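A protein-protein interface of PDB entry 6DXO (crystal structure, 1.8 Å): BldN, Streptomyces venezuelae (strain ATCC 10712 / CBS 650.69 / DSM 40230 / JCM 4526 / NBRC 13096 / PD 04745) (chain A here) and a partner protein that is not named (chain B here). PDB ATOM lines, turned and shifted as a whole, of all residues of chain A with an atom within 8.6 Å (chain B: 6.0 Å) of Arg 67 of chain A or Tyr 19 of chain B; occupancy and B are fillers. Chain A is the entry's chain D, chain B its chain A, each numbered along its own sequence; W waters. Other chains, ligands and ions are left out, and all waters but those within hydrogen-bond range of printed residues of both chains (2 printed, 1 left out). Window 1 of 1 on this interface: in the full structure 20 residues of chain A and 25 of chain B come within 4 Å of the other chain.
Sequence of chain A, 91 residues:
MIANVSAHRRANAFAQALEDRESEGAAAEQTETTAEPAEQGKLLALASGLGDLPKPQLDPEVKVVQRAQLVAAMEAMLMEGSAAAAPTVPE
The side-chain carboxylate (OD1) of Asp 20 of chain B is in salt-bridge range of the guanidinium group (NE) of Arg 67 of chain A, at 2.9 Å.
NH2 of Arg 67 of chain A lies within salt-bridge range of OE2 of Glu 13 of chain B (2.6 Å).
OE1 of Gln 66 of chain A is in hydrogen-bond range of OH of Tyr 19 of chain B (2.7 Å).
The side-chain carboxylate (OD1) of Asp 24 of chain B lies within salt-bridge range of the side-chain amino group (NZ) of Lys 63 of chain A (3.0 Å).
NZ of Lys 63 of chain A is in hydrogen-bond range of OG of Ser 23 of chain B (2.5 Å).
The guanidinium group (NH2) of Arg 17 of chain B is in salt-bridge range of the side-chain carboxylate (OD2) of Asp 20 of chain B (3.1 Å).
O of Tyr 19 of chain B is in hydrogen-bond range of OG of Ser 23 of chain B, 3.0 Å away.
OH of Tyr 19 of chain B touches CD1 of Leu 58 of chain A (3.5 Å).
Ser 45 of chain B touches Gln 66 of chain A (CB to NE2, 3.5 Å).
NH2 of Arg 67 of chain A touches C of Gly 16 of chain B (3.4 Å).
Arg 17 of chain B touches Arg 67 of chain A (N to NH2, 3.6 Å).
Tyr 19 of chain B touches Arg 67 of chain A.
CD2 of Leu 70 of chain A touches CE2 of Phe 15 of chain B, 3.7 Å away.
Tyr 19 of chain B touches Leu 70 of chain A.
CB of Phe 48 of chain B touches CD2 of Leu 70 of chain A, at 3.7 Å.
CA of Gly 16 of chain B touches CG2 of Val 71 of chain A (3.95 Å).
CG of Met 74 of chain A touches CB of Phe 15 of chain B, 3.95 Å away.
Printed residues of chain B within 4 Å of Leu 58 of chain A: Tyr 19 (3.5 Å), Ser 23 (3.9 Å) and Asp 24 (3.6 Å).
Pro 60 of chain A touches none of the printed residues of chain B.
Of chain B, only Glu 13, Gly 16, Arg 17, Tyr 19 and Asp 20 come within 4 Å of Arg 67 of chain A.
Ala 68 of chain A touches none of the printed residues of chain B.
Tyr 19 of chain B touches just these residues of chain A: Leu 58 (3.5 Å), Lys 63 (3.5 Å), Gln 66 (2.7 Å), Arg 67 (3.9 Å) and Leu 70 (3.4 Å).
Of the printed residues of chain A, Ser 23 of chain B touches Leu 58 (3.9 Å) and Lys 63 (2.5 Å).
The nearest printed residue of chain B that does not touch Arg 67 of chain A is Phe 15 of chain B (6.0 Å).
The nearest printed residue of chain A that does not touch Phe 15 of chain B is Val 71 of chain A (5.3 Å).
Of the 15 printed residues of chain B, 10 touch a printed residue of chain A.
Printed residues of chain B that touch a printed residue of chain A: Glu 13, Phe 15, Gly 16, Arg 17, Tyr 19, Asp 20, Ser 23, Asp 24, Ser 45 and Phe 48.
Hydrophobic or aromatic side chains of chain B within 4 Å of the printed part of chain A: Phe 15, Tyr 19 and Phe 48.
Of the 17 printed residues of chain A, 7 touch a printed residue of chain B.
Among the printed residues, Asp or Glu carboxylates within 4 Å of a Lys or Arg side-chain nitrogen of the other chain: Lys 63 of chain A with Asp 24 of chain B (3.0 Å), Arg 67 of chain A with Glu 13 of chain B (2.6 Å) and Arg 67 of chain A with Asp 20 of chain B (2.9 Å).
Water W2 lies within hydrogen-bond range of OG of Ser 45 of chain B (2.5 Å), NE2 of Gln 69 of chain A (2.8 Å) and O of Gln 66 of chain A (3.4 Å).
Water W1 lies within hydrogen-bond range of NZ of Lys 63 of chain A (2.8 Å) and O of Asp 20 of chain B (2.9 Å).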
ATOM      1  N   LEU A  58      -4.776  32.496   9.818  1.00  0.00           N
ATOM      2  CA  LEU A  58      -4.389  31.448   8.883  1.00  0.00           C
ATOM      3  C   LEU A  58      -5.283  30.253   9.130  1.00  0.00           C
ATOM      4  O   LEU A  58      -5.466  29.860  10.279  1.00  0.00           O
ATOM      5  CB  LEU A  58      -2.943  31.022   9.134  1.00  0.00           C
ATOM      6  CG  LEU A  58      -1.818  31.450   8.197  1.00  0.00           C
ATOM      7  CD1 LEU A  58      -0.470  30.973   8.744  1.00  0.00           C
ATOM      8  CD2 LEU A  58      -2.054  30.921   6.803  1.00  0.00           C
ATOM      9  N   ASP A  59      -5.835  29.693   8.056  1.00  0.00           N
ATOM     10  CA  ASP A  59      -6.677  28.508   8.125  1.00  0.00           C
ATOM     11  C   ASP A  59      -5.972  27.407   8.920  1.00  0.00           C
ATOM     12  O   ASP A  59      -4.845  27.062   8.619  1.00  0.00           O
ATOM     13  CB  ASP A  59      -6.930  28.038   6.692  1.00  0.00           C
ATOM     14  CG  ASP A  59      -7.855  26.852   6.611  1.00  0.00           C
ATOM     15  OD1 ASP A  59      -7.857  26.026   7.541  1.00  0.00           O
ATOM     16  OD2 ASP A  59      -8.576  26.738   5.595  1.00  0.00           O
ATOM     17  N   PRO A  60      -6.650  26.844   9.927  1.00  0.00           N
ATOM     18  CA  PRO A  60      -6.026  25.740  10.678  1.00  0.00           C
ATOM     19  C   PRO A  60      -5.503  24.617   9.802  1.00  0.00           C
ATOM     20  O   PRO A  60      -4.397  24.153  10.042  1.00  0.00           O
ATOM     21  CB  PRO A  60      -7.162  25.226  11.561  1.00  0.00           C
ATOM     22  CG  PRO A  60      -8.052  26.402  11.749  1.00  0.00           C
ATOM     23  CD  PRO A  60      -7.965  27.215  10.478  1.00  0.00           C
ATOM     24  N   GLU A  61      -6.266  24.155   8.812  1.00  0.00           N
ATOM     25  CA  GLU A  61      -5.767  23.039   8.014  1.00  0.00           C
ATOM     26  C   GLU A  61      -4.590  23.417   7.109  1.00  0.00           C
ATOM     27  O   GLU A  61      -3.731  22.590   6.805  1.00  0.00           O
ATOM     28  CB  GLU A  61      -6.900  22.341   7.251  1.00  0.00           C
ATOM     29  CG  GLU A  61      -7.897  21.649   8.196  1.00  0.00           C
ATOM     30  CD  GLU A  61      -7.221  20.790   9.274  1.00  0.00           C
ATOM     31  OE1 GLU A  61      -6.547  19.805   8.914  1.00  0.00           O
ATOM     32  OE2 GLU A  61      -7.365  21.092  10.483  1.00  0.00           O
ATOM     33  N   VAL A  62      -4.527  24.680   6.706  1.00  0.00           N
ATOM     34  CA  VAL A  62      -3.324  25.175   6.034  1.00  0.00           C
ATOM     35  C   VAL A  62      -2.096  25.164   6.968  1.00  0.00           C
ATOM     36  O   VAL A  62      -1.001  24.772   6.558  1.00  0.00           O
ATOM     37  CB  VAL A  62      -3.559  26.578   5.471  1.00  0.00           C
ATOM     38  CG1 VAL A  62      -2.281  27.149   4.886  1.00  0.00           C
ATOM     39  CG2 VAL A  62      -4.666  26.513   4.419  1.00  0.00           C
ATOM     40  N   LYS A  63      -2.272  25.610   8.207  1.00  0.00           N
ATOM     41  CA  LYS A  63      -1.171  25.531   9.180  1.00  0.00           C
ATOM     42  C   LYS A  63      -0.612  24.114   9.314  1.00  0.00           C
ATOM     43  O   LYS A  63       0.608  23.916   9.465  1.00  0.00           O
ATOM     44  CB  LYS A  63      -1.616  26.030  10.552  1.00  0.00           C
ATOM     45  CG  LYS A  63      -1.819  27.527  10.656  1.00  0.00           C
ATOM     46  CD  LYS A  63      -1.971  27.894  12.132  1.00  0.00           C
ATOM     47  CE  LYS A  63      -2.013  29.394  12.355  1.00  0.00           C
ATOM     48  NZ  LYS A  63      -0.646  29.934  12.571  1.00  0.00           N
ATOM     49  N   VAL A  64      -1.495  23.116   9.321  1.00  0.00           N
ATOM     50  CA  VAL A  64      -1.010  21.744   9.470  1.00  0.00           C
ATOM     51  C   VAL A  64      -0.018  21.401   8.359  1.00  0.00           C
ATOM     52  O   VAL A  64       1.066  20.873   8.608  1.00  0.00           O
ATOM     53  CB  VAL A  64      -2.163  20.719   9.468  1.00  0.00           C
ATOM     54  CG1 VAL A  64      -1.604  19.306   9.653  1.00  0.00           C
ATOM     55  CG2 VAL A  64      -3.159  21.071  10.561  1.00  0.00           C
ATOM     56  N   VAL A  65      -0.373  21.748   7.128  1.00  0.00           N
ATOM     57  CA  VAL A  65       0.427  21.349   5.985  1.00  0.00           C
ATOM     58  C   VAL A  65       1.712  22.166   5.927  1.00  0.00           C
ATOM     59  O   VAL A  65       2.808  21.620   5.703  1.00  0.00           O
ATOM     60  CB  VAL A  65      -0.348  21.489   4.668  1.00  0.00           C
ATOM     61  CG1 VAL A  65       0.556  21.213   3.488  1.00  0.00           C
ATOM     62  CG2 VAL A  65      -1.543  20.514   4.637  1.00  0.00           C
ATOM     63  N   GLN A  66       1.592  23.466   6.163  1.00  0.00           N
ATOM     64  CA  GLN A  66       2.792  24.318   6.120  1.00  0.00           C
ATOM     65  C   GLN A  66       3.800  23.916   7.187  1.00  0.00           C
ATOM     66  O   GLN A  66       4.998  23.860   6.927  1.00  0.00           O
ATOM     67  CB  GLN A  66       2.437  25.790   6.277  1.00  0.00           C
ATOM     68  CG  GLN A  66       1.563  26.300   5.131  1.00  0.00           C
ATOM     69  CD  GLN A  66       1.420  27.820   5.095  1.00  0.00           C
ATOM     70  OE1 GLN A  66       1.600  28.513   6.106  1.00  0.00           O
ATOM     71  NE2 GLN A  66       1.063  28.340   3.927  1.00  0.00           N
ATOM     72  N   ARG A  67       3.318  23.687   8.401  1.00  0.00           N
ATOM     73  CA  ARG A  67       4.199  23.281   9.499  1.00  0.00           C
ATOM     74  C   ARG A  67       4.919  21.978   9.159  1.00  0.00           C
ATOM     75  O   ARG A  67       6.117  21.831   9.420  1.00  0.00           O
ATOM     76  CB  ARG A  67       3.406  23.139  10.812  1.00  0.00           C
ATOM     77  CG  ARG A  67       4.295  22.995  12.078  1.00  0.00           C
ATOM     78  CD  ARG A  67       3.471  22.594  13.304  1.00  0.00           C
ATOM     79  NE  ARG A  67       4.135  22.918  14.564  1.00  0.00           N
ATOM     80  CZ  ARG A  67       5.032  22.140  15.172  1.00  0.00           C
ATOM     81  NH1 ARG A  67       5.378  20.980  14.636  1.00  0.00           N
ATOM     82  NH2 ARG A  67       5.600  22.539  16.305  1.00  0.00           N
ATOM     83  N   ALA A  68       4.180  21.019   8.606  1.00  0.00           N
ATOM     84  CA  ALA A  68       4.763  19.739   8.233  1.00  0.00           C
ATOM     85  C   ALA A  68       5.797  19.931   7.121  1.00  0.00           C
ATOM     86  O   ALA A  68       6.879  19.341   7.153  1.00  0.00           O
ATOM     87  CB  ALA A  68       3.677  18.748   7.807  1.00  0.00           C
ATOM     88  N   GLN A  69       5.477  20.780   6.146  1.00  0.00           N
ATOM     89  CA  GLN A  69       6.440  21.099   5.089  1.00  0.00           C
ATOM     90  C   GLN A  69       7.731  21.677   5.675  1.00  0.00           C
ATOM     91  O   GLN A  69       8.826  21.367   5.206  1.00  0.00           O
ATOM     92  CB  GLN A  69       5.854  22.103   4.088  1.00  0.00           C
ATOM     93  CG  GLN A  69       4.921  21.510   3.034  1.00  0.00           C
ATOM     94  CD  GLN A  69       4.420  22.559   2.051  1.00  0.00           C
ATOM     95  OE1 GLN A  69       4.675  22.477   0.847  1.00  0.00           O
ATOM     96  NE2 GLN A  69       3.705  23.556   2.566  1.00  0.00           N
ATOM     97  N   LEU A  70       7.614  22.519   6.691  1.00  0.00           N
ATOM     98  CA  LEU A  70       8.817  23.159   7.236  1.00  0.00           C
ATOM     99  C   LEU A  70       9.661  22.195   8.073  1.00  0.00           C
ATOM    100  O   LEU A  70      10.906  22.195   8.007  1.00  0.00           O
ATOM    101  CB  LEU A  70       8.416  24.371   8.060  1.00  0.00           C
ATOM    102  CG  LEU A  70       7.821  25.456   7.172  1.00  0.00           C
ATOM    103  CD1 LEU A  70       6.912  26.379   7.946  1.00  0.00           C
ATOM    104  CD2 LEU A  70       9.007  26.254   6.533  1.00  0.00           C
ATOM    105  N   VAL A  71       8.990  21.371   8.862  1.00  0.00           N
ATOM    106  CA  VAL A  71       9.689  20.391   9.684  1.00  0.00           C
ATOM    107  C   VAL A  71      10.407  19.385   8.785  1.00  0.00           C
ATOM    108  O   VAL A  71      11.551  19.017   9.049  1.00  0.00           O
ATOM    109  CB  VAL A  71       8.726  19.684  10.689  1.00  0.00           C
ATOM    110  CG1 VAL A  71       9.446  18.568  11.445  1.00  0.00           C
ATOM    111  CG2 VAL A  71       8.179  20.700  11.683  1.00  0.00           C
ATOM    112  N   ALA A  72       9.738  18.960   7.715  1.00  0.00           N
ATOM    113  CA  ALA A  72      10.340  18.060   6.733  1.00  0.00           C
ATOM    114  C   ALA A  72      11.538  18.708   6.030  1.00  0.00           C
ATOM    115  O   ALA A  72      12.583  18.084   5.877  1.00  0.00           O
ATOM    116  CB  ALA A  72       9.299  17.605   5.715  1.00  0.00           C
ATOM    117  N   ALA A  73      11.385  19.956   5.589  1.00  0.00           N
ATOM    118  CA  ALA A  73      12.497  20.657   4.943  1.00  0.00           C
ATOM    119  C   ALA A  73      13.709  20.691   5.860  1.00  0.00           C
ATOM    120  O   ALA A  73      14.840  20.527   5.407  1.00  0.00           O
ATOM    121  CB  ALA A  73      12.090  22.056   4.552  1.00  0.00           C
ATOM    122  N   MET A  74      13.474  20.904   7.152  1.00  0.00           N
ATOM    123  CA  MET A  74      14.550  20.917   8.138  1.00  0.00           C
ATOM    124  C   MET A  74      15.216  19.557   8.271  1.00  0.00           C
ATOM    125  O   MET A  74      16.449  19.453   8.276  1.00  0.00           O
ATOM    126  CB  MET A  74      14.039  21.369   9.509  1.00  0.00           C
ATOM    127  CG  MET A  74      14.480  22.768   9.920  1.00  0.00           C
ATOM    128  SD  MET A  74      16.274  22.943   9.954  1.00  0.00           S
ATOM    129  CE  MET A  74      16.757  21.422  10.764  1.00  0.00           C
ATOM    130  N   GLU B  13      11.860  20.235  15.104  1.00  0.00           N
ATOM    131  CA  GLU B  13      10.661  20.638  15.835  1.00  0.00           C
ATOM    132  C   GLU B  13      10.771  22.056  16.403  1.00  0.00           C
ATOM    133  O   GLU B  13       9.763  22.747  16.554  1.00  0.00           O
ATOM    134  CB  GLU B  13      10.328  19.634  16.944  1.00  0.00           C
ATOM    135  CG  GLU B  13       9.261  20.122  17.917  1.00  0.00           C
ATOM    136  CD  GLU B  13       7.892  20.308  17.266  1.00  0.00           C
ATOM    137  OE1 GLU B  13       7.665  19.757  16.169  1.00  0.00           O
ATOM    138  OE2 GLU B  13       7.048  21.013  17.855  1.00  0.00           O
ATOM    139  N   ALA B  14      11.990  22.494  16.714  1.00  0.00           N
ATOM    140  CA  ALA B  14      12.186  23.862  17.151  1.00  0.00           C
ATOM    141  C   ALA B  14      11.771  24.824  16.041  1.00  0.00           C
ATOM    142  O   ALA B  14      11.155  25.852  16.315  1.00  0.00           O
ATOM    143  CB  ALA B  14      13.653  24.126  17.586  1.00  0.00           C
ATOM    144  N   PHE B  15      12.074  24.485  14.790  1.00  0.00           N
ATOM    145  CA  PHE B  15      11.654  25.362  13.692  1.00  0.00           C
ATOM    146  C   PHE B  15      10.127  25.291  13.536  1.00  0.00           C
ATOM    147  O   PHE B  15       9.473  26.267  13.216  1.00  0.00           O
ATOM    148  CB  PHE B  15      12.332  25.014  12.366  1.00  0.00           C
ATOM    149  CG  PHE B  15      12.197  26.099  11.339  1.00  0.00           C
ATOM    150  CD1 PHE B  15      13.121  27.132  11.281  1.00  0.00           C
ATOM    151  CD2 PHE B  15      11.122  26.114  10.456  1.00  0.00           C
ATOM    152  CE1 PHE B  15      12.990  28.155  10.334  1.00  0.00           C
ATOM    153  CE2 PHE B  15      10.978  27.141   9.516  1.00  0.00           C
ATOM    154  CZ  PHE B  15      11.905  28.156   9.468  1.00  0.00           C
ATOM    155  N   GLY B  16       9.558  24.128  13.794  1.00  0.00           N
ATOM    156  CA  GLY B  16       8.098  24.031  13.808  1.00  0.00           C
ATOM    157  C   GLY B  16       7.485  24.979  14.824  1.00  0.00           C
ATOM    158  O   GLY B  16       6.466  25.646  14.566  1.00  0.00           O
ATOM    159  N   ARG B  17       8.098  25.045  15.997  1.00  0.00           N
ATOM    160  CA  ARG B  17       7.671  25.963  17.037  1.00  0.00           C
ATOM    161  C   ARG B  17       7.832  27.434  16.618  1.00  0.00           C
ATOM    162  O   ARG B  17       7.038  28.292  17.017  1.00  0.00           O
ATOM    163  CB  ARG B  17       8.480  25.718  18.311  1.00  0.00           C
ATOM    164  CG  ARG B  17       8.391  24.294  18.829  1.00  0.00           C
ATOM    165  CD  ARG B  17       7.425  24.205  19.995  1.00  0.00           C
ATOM    166  NE  ARG B  17       6.142  24.814  19.675  1.00  0.00           N
ATOM    167  CZ  ARG B  17       5.530  25.712  20.436  1.00  0.00           C
ATOM    168  NH1 ARG B  17       6.081  26.108  21.574  1.00  0.00           N
ATOM    169  NH2 ARG B  17       4.361  26.212  20.061  1.00  0.00           N
ATOM    170  N   LEU B  18       8.871  27.740  15.850  1.00  0.00           N
ATOM    171  CA  LEU B  18       9.026  29.112  15.366  1.00  0.00           C
ATOM    172  C   LEU B  18       7.838  29.442  14.450  1.00  0.00           C
ATOM    173  O   LEU B  18       7.263  30.525  14.540  1.00  0.00           O
ATOM    174  CB  LEU B  18      10.365  29.327  14.646  1.00  0.00           C
ATOM    175  CG  LEU B  18      11.602  29.363  15.562  1.00  0.00           C
ATOM    176  CD1 LEU B  18      12.891  29.441  14.749  1.00  0.00           C
ATOM    177  CD2 LEU B  18      11.492  30.507  16.550  1.00  0.00           C
ATOM    178  N   TYR B  19       7.475  28.507  13.583  1.00  0.00           N
ATOM    179  CA  TYR B  19       6.267  28.659  12.772  1.00  0.00           C
ATOM    180  C   TYR B  19       5.025  28.890  13.628  1.00  0.00           C
ATOM    181  O   TYR B  19       4.252  29.817  13.383  1.00  0.00           O
ATOM    182  CB  TYR B  19       6.082  27.472  11.828  1.00  0.00           C
ATOM    183  CG  TYR B  19       4.810  27.584  11.006  1.00  0.00           C
ATOM    184  CD1 TYR B  19       4.796  28.305   9.818  1.00  0.00           C
ATOM    185  CD2 TYR B  19       3.631  26.997  11.440  1.00  0.00           C
ATOM    186  CE1 TYR B  19       3.626  28.433   9.062  1.00  0.00           C
ATOM    187  CE2 TYR B  19       2.455  27.111  10.695  1.00  0.00           C
ATOM    188  CZ  TYR B  19       2.465  27.822   9.506  1.00  0.00           C
ATOM    189  OH  TYR B  19       1.304  27.940   8.777  1.00  0.00           O
ATOM    190  N   ASP B  20       4.822  28.057  14.650  1.00  0.00           N
ATOM    191  CA  ASP B  20       3.721  28.300  15.576  1.00  0.00           C
ATOM    192  C   ASP B  20       3.685  29.726  16.129  1.00  0.00           C
ATOM    193  O   ASP B  20       2.632  30.361  16.183  1.00  0.00           O
ATOM    194  CB  ASP B  20       3.790  27.332  16.760  1.00  0.00           C
ATOM    195  CG  ASP B  20       3.691  25.892  16.351  1.00  0.00           C
ATOM    196  OD1 ASP B  20       3.171  25.579  15.257  1.00  0.00           O
ATOM    197  OD2 ASP B  20       4.134  25.044  17.170  1.00  0.00           O
ATOM    198  N   GLN B  21       4.841  30.245  16.525  1.00  0.00           N
ATOM    199  CA  GLN B  21       4.917  31.521  17.212  1.00  0.00           C
ATOM    200  C   GLN B  21       4.689  32.715  16.259  1.00  0.00           C
ATOM    201  O   GLN B  21       4.063  33.707  16.630  1.00  0.00           O
ATOM    202  CB  GLN B  21       6.306  31.654  17.860  1.00  0.00           C
ATOM    203  CG  GLN B  21       6.627  32.997  18.498  1.00  0.00           C
ATOM    204  CD  GLN B  21       7.956  32.966  19.256  1.00  0.00           C
ATOM    205  OE1 GLN B  21       8.578  31.913  19.406  1.00  0.00           O
ATOM    206  NE2 GLN B  21       8.392  34.129  19.736  1.00  0.00           N
ATOM    207  N   TYR B  22       5.188  32.592  15.038  1.00  0.00           N
ATOM    208  CA  TYR B  22       5.269  33.749  14.134  1.00  0.00           C
ATOM    209  C   TYR B  22       4.364  33.687  12.907  1.00  0.00           C
ATOM    210  O   TYR B  22       4.232  34.694  12.190  1.00  0.00           O
ATOM    211  CB  TYR B  22       6.711  33.937  13.647  1.00  0.00           C
ATOM    212  CG  TYR B  22       7.651  34.413  14.704  1.00  0.00           C
ATOM    213  CD1 TYR B  22       8.555  33.537  15.291  1.00  0.00           C
ATOM    214  CD2 TYR B  22       7.659  35.747  15.112  1.00  0.00           C
ATOM    215  CE1 TYR B  22       9.461  33.975  16.267  1.00  0.00           C
ATOM    216  CE2 TYR B  22       8.579  36.197  16.097  1.00  0.00           C
ATOM    217  CZ  TYR B  22       9.459  35.298  16.666  1.00  0.00           C
ATOM    218  OH  TYR B  22      10.366  35.718  17.628  1.00  0.00           O
ATOM    219  N   SER B  23       3.760  32.536  12.627  1.00  0.00           N
ATOM    220  CA  SER B  23       3.063  32.404  11.339  1.00  0.00           C
ATOM    221  C   SER B  23       1.912  33.379  11.167  1.00  0.00           C
ATOM    222  O   SER B  23       1.743  33.942  10.077  1.00  0.00           O
ATOM    223  CB  SER B  23       2.598  30.966  11.071  1.00  0.00           C
ATOM    224  OG  SER B  23       1.702  30.549  12.071  1.00  0.00           O
ATOM    225  N   ASP B  24       1.132  33.612  12.224  1.00  0.00           N
ATOM    226  CA  ASP B  24      -0.051  34.478  12.081  1.00  0.00           C
ATOM    227  C   ASP B  24       0.363  35.928  11.836  1.00  0.00           C
ATOM    228  O   ASP B  24      -0.280  36.663  11.084  1.00  0.00           O
ATOM    229  CB  ASP B  24      -0.956  34.400  13.311  1.00  0.00           C
ATOM    230  CG  ASP B  24      -1.747  33.093  13.386  1.00  0.00           C
ATOM    231  OD1 ASP B  24      -2.080  32.510  12.327  1.00  0.00           O
ATOM    232  OD2 ASP B  24      -2.059  32.662  14.512  1.00  0.00           O
ATOM    233  N   THR B  44       3.309  33.096   2.807  1.00  0.00           N
ATOM    234  CA  THR B  44       3.640  32.889   4.217  1.00  0.00           C
ATOM    235  C   THR B  44       4.550  31.680   4.291  1.00  0.00           C
ATOM    236  O   THR B  44       5.604  31.703   4.943  1.00  0.00           O
ATOM    237  CB  THR B  44       2.355  32.680   5.073  1.00  0.00           C
ATOM    238  OG1 THR B  44       1.570  33.877   5.040  1.00  0.00           O
ATOM    239  CG2 THR B  44       2.721  32.386   6.527  1.00  0.00           C
ATOM    240  N   SER B  45       4.155  30.627   3.589  1.00  0.00           N
ATOM    241  CA  SER B  45       4.963  29.416   3.493  1.00  0.00           C
ATOM    242  C   SER B  45       6.330  29.737   2.917  1.00  0.00           C
ATOM    243  O   SER B  45       7.351  29.354   3.478  1.00  0.00           O
ATOM    244  CB  SER B  45       4.255  28.385   2.614  1.00  0.00           C
ATOM    245  OG  SER B  45       5.109  27.300   2.314  1.00  0.00           O
ATOM    246  N   PHE B  48       8.760  31.544   5.455  1.00  0.00           N
ATOM    247  CA  PHE B  48       9.421  30.632   6.380  1.00  0.00           C
ATOM    248  C   PHE B  48      10.455  29.724   5.708  1.00  0.00           C
ATOM    249  O   PHE B  48      11.522  29.441   6.287  1.00  0.00           O
ATOM    250  CB  PHE B  48       8.387  29.815   7.160  1.00  0.00           C
ATOM    251  CG  PHE B  48       7.725  30.591   8.247  1.00  0.00           C
ATOM    252  CD1 PHE B  48       6.544  31.302   8.003  1.00  0.00           C
ATOM    253  CD2 PHE B  48       8.286  30.641   9.513  1.00  0.00           C
ATOM    254  CE1 PHE B  48       5.942  32.038   9.020  1.00  0.00           C
ATOM    255  CE2 PHE B  48       7.682  31.363  10.537  1.00  0.00           C
ATOM    256  CZ  PHE B  48       6.506  32.069  10.295  1.00  0.00           C
HETATM  257  O   HOH W   1       0.259  29.052  15.039  1.00  0.00           O
HETATM  258  O   HOH W   2       5.320  25.372   3.881  1.00  0.00           O
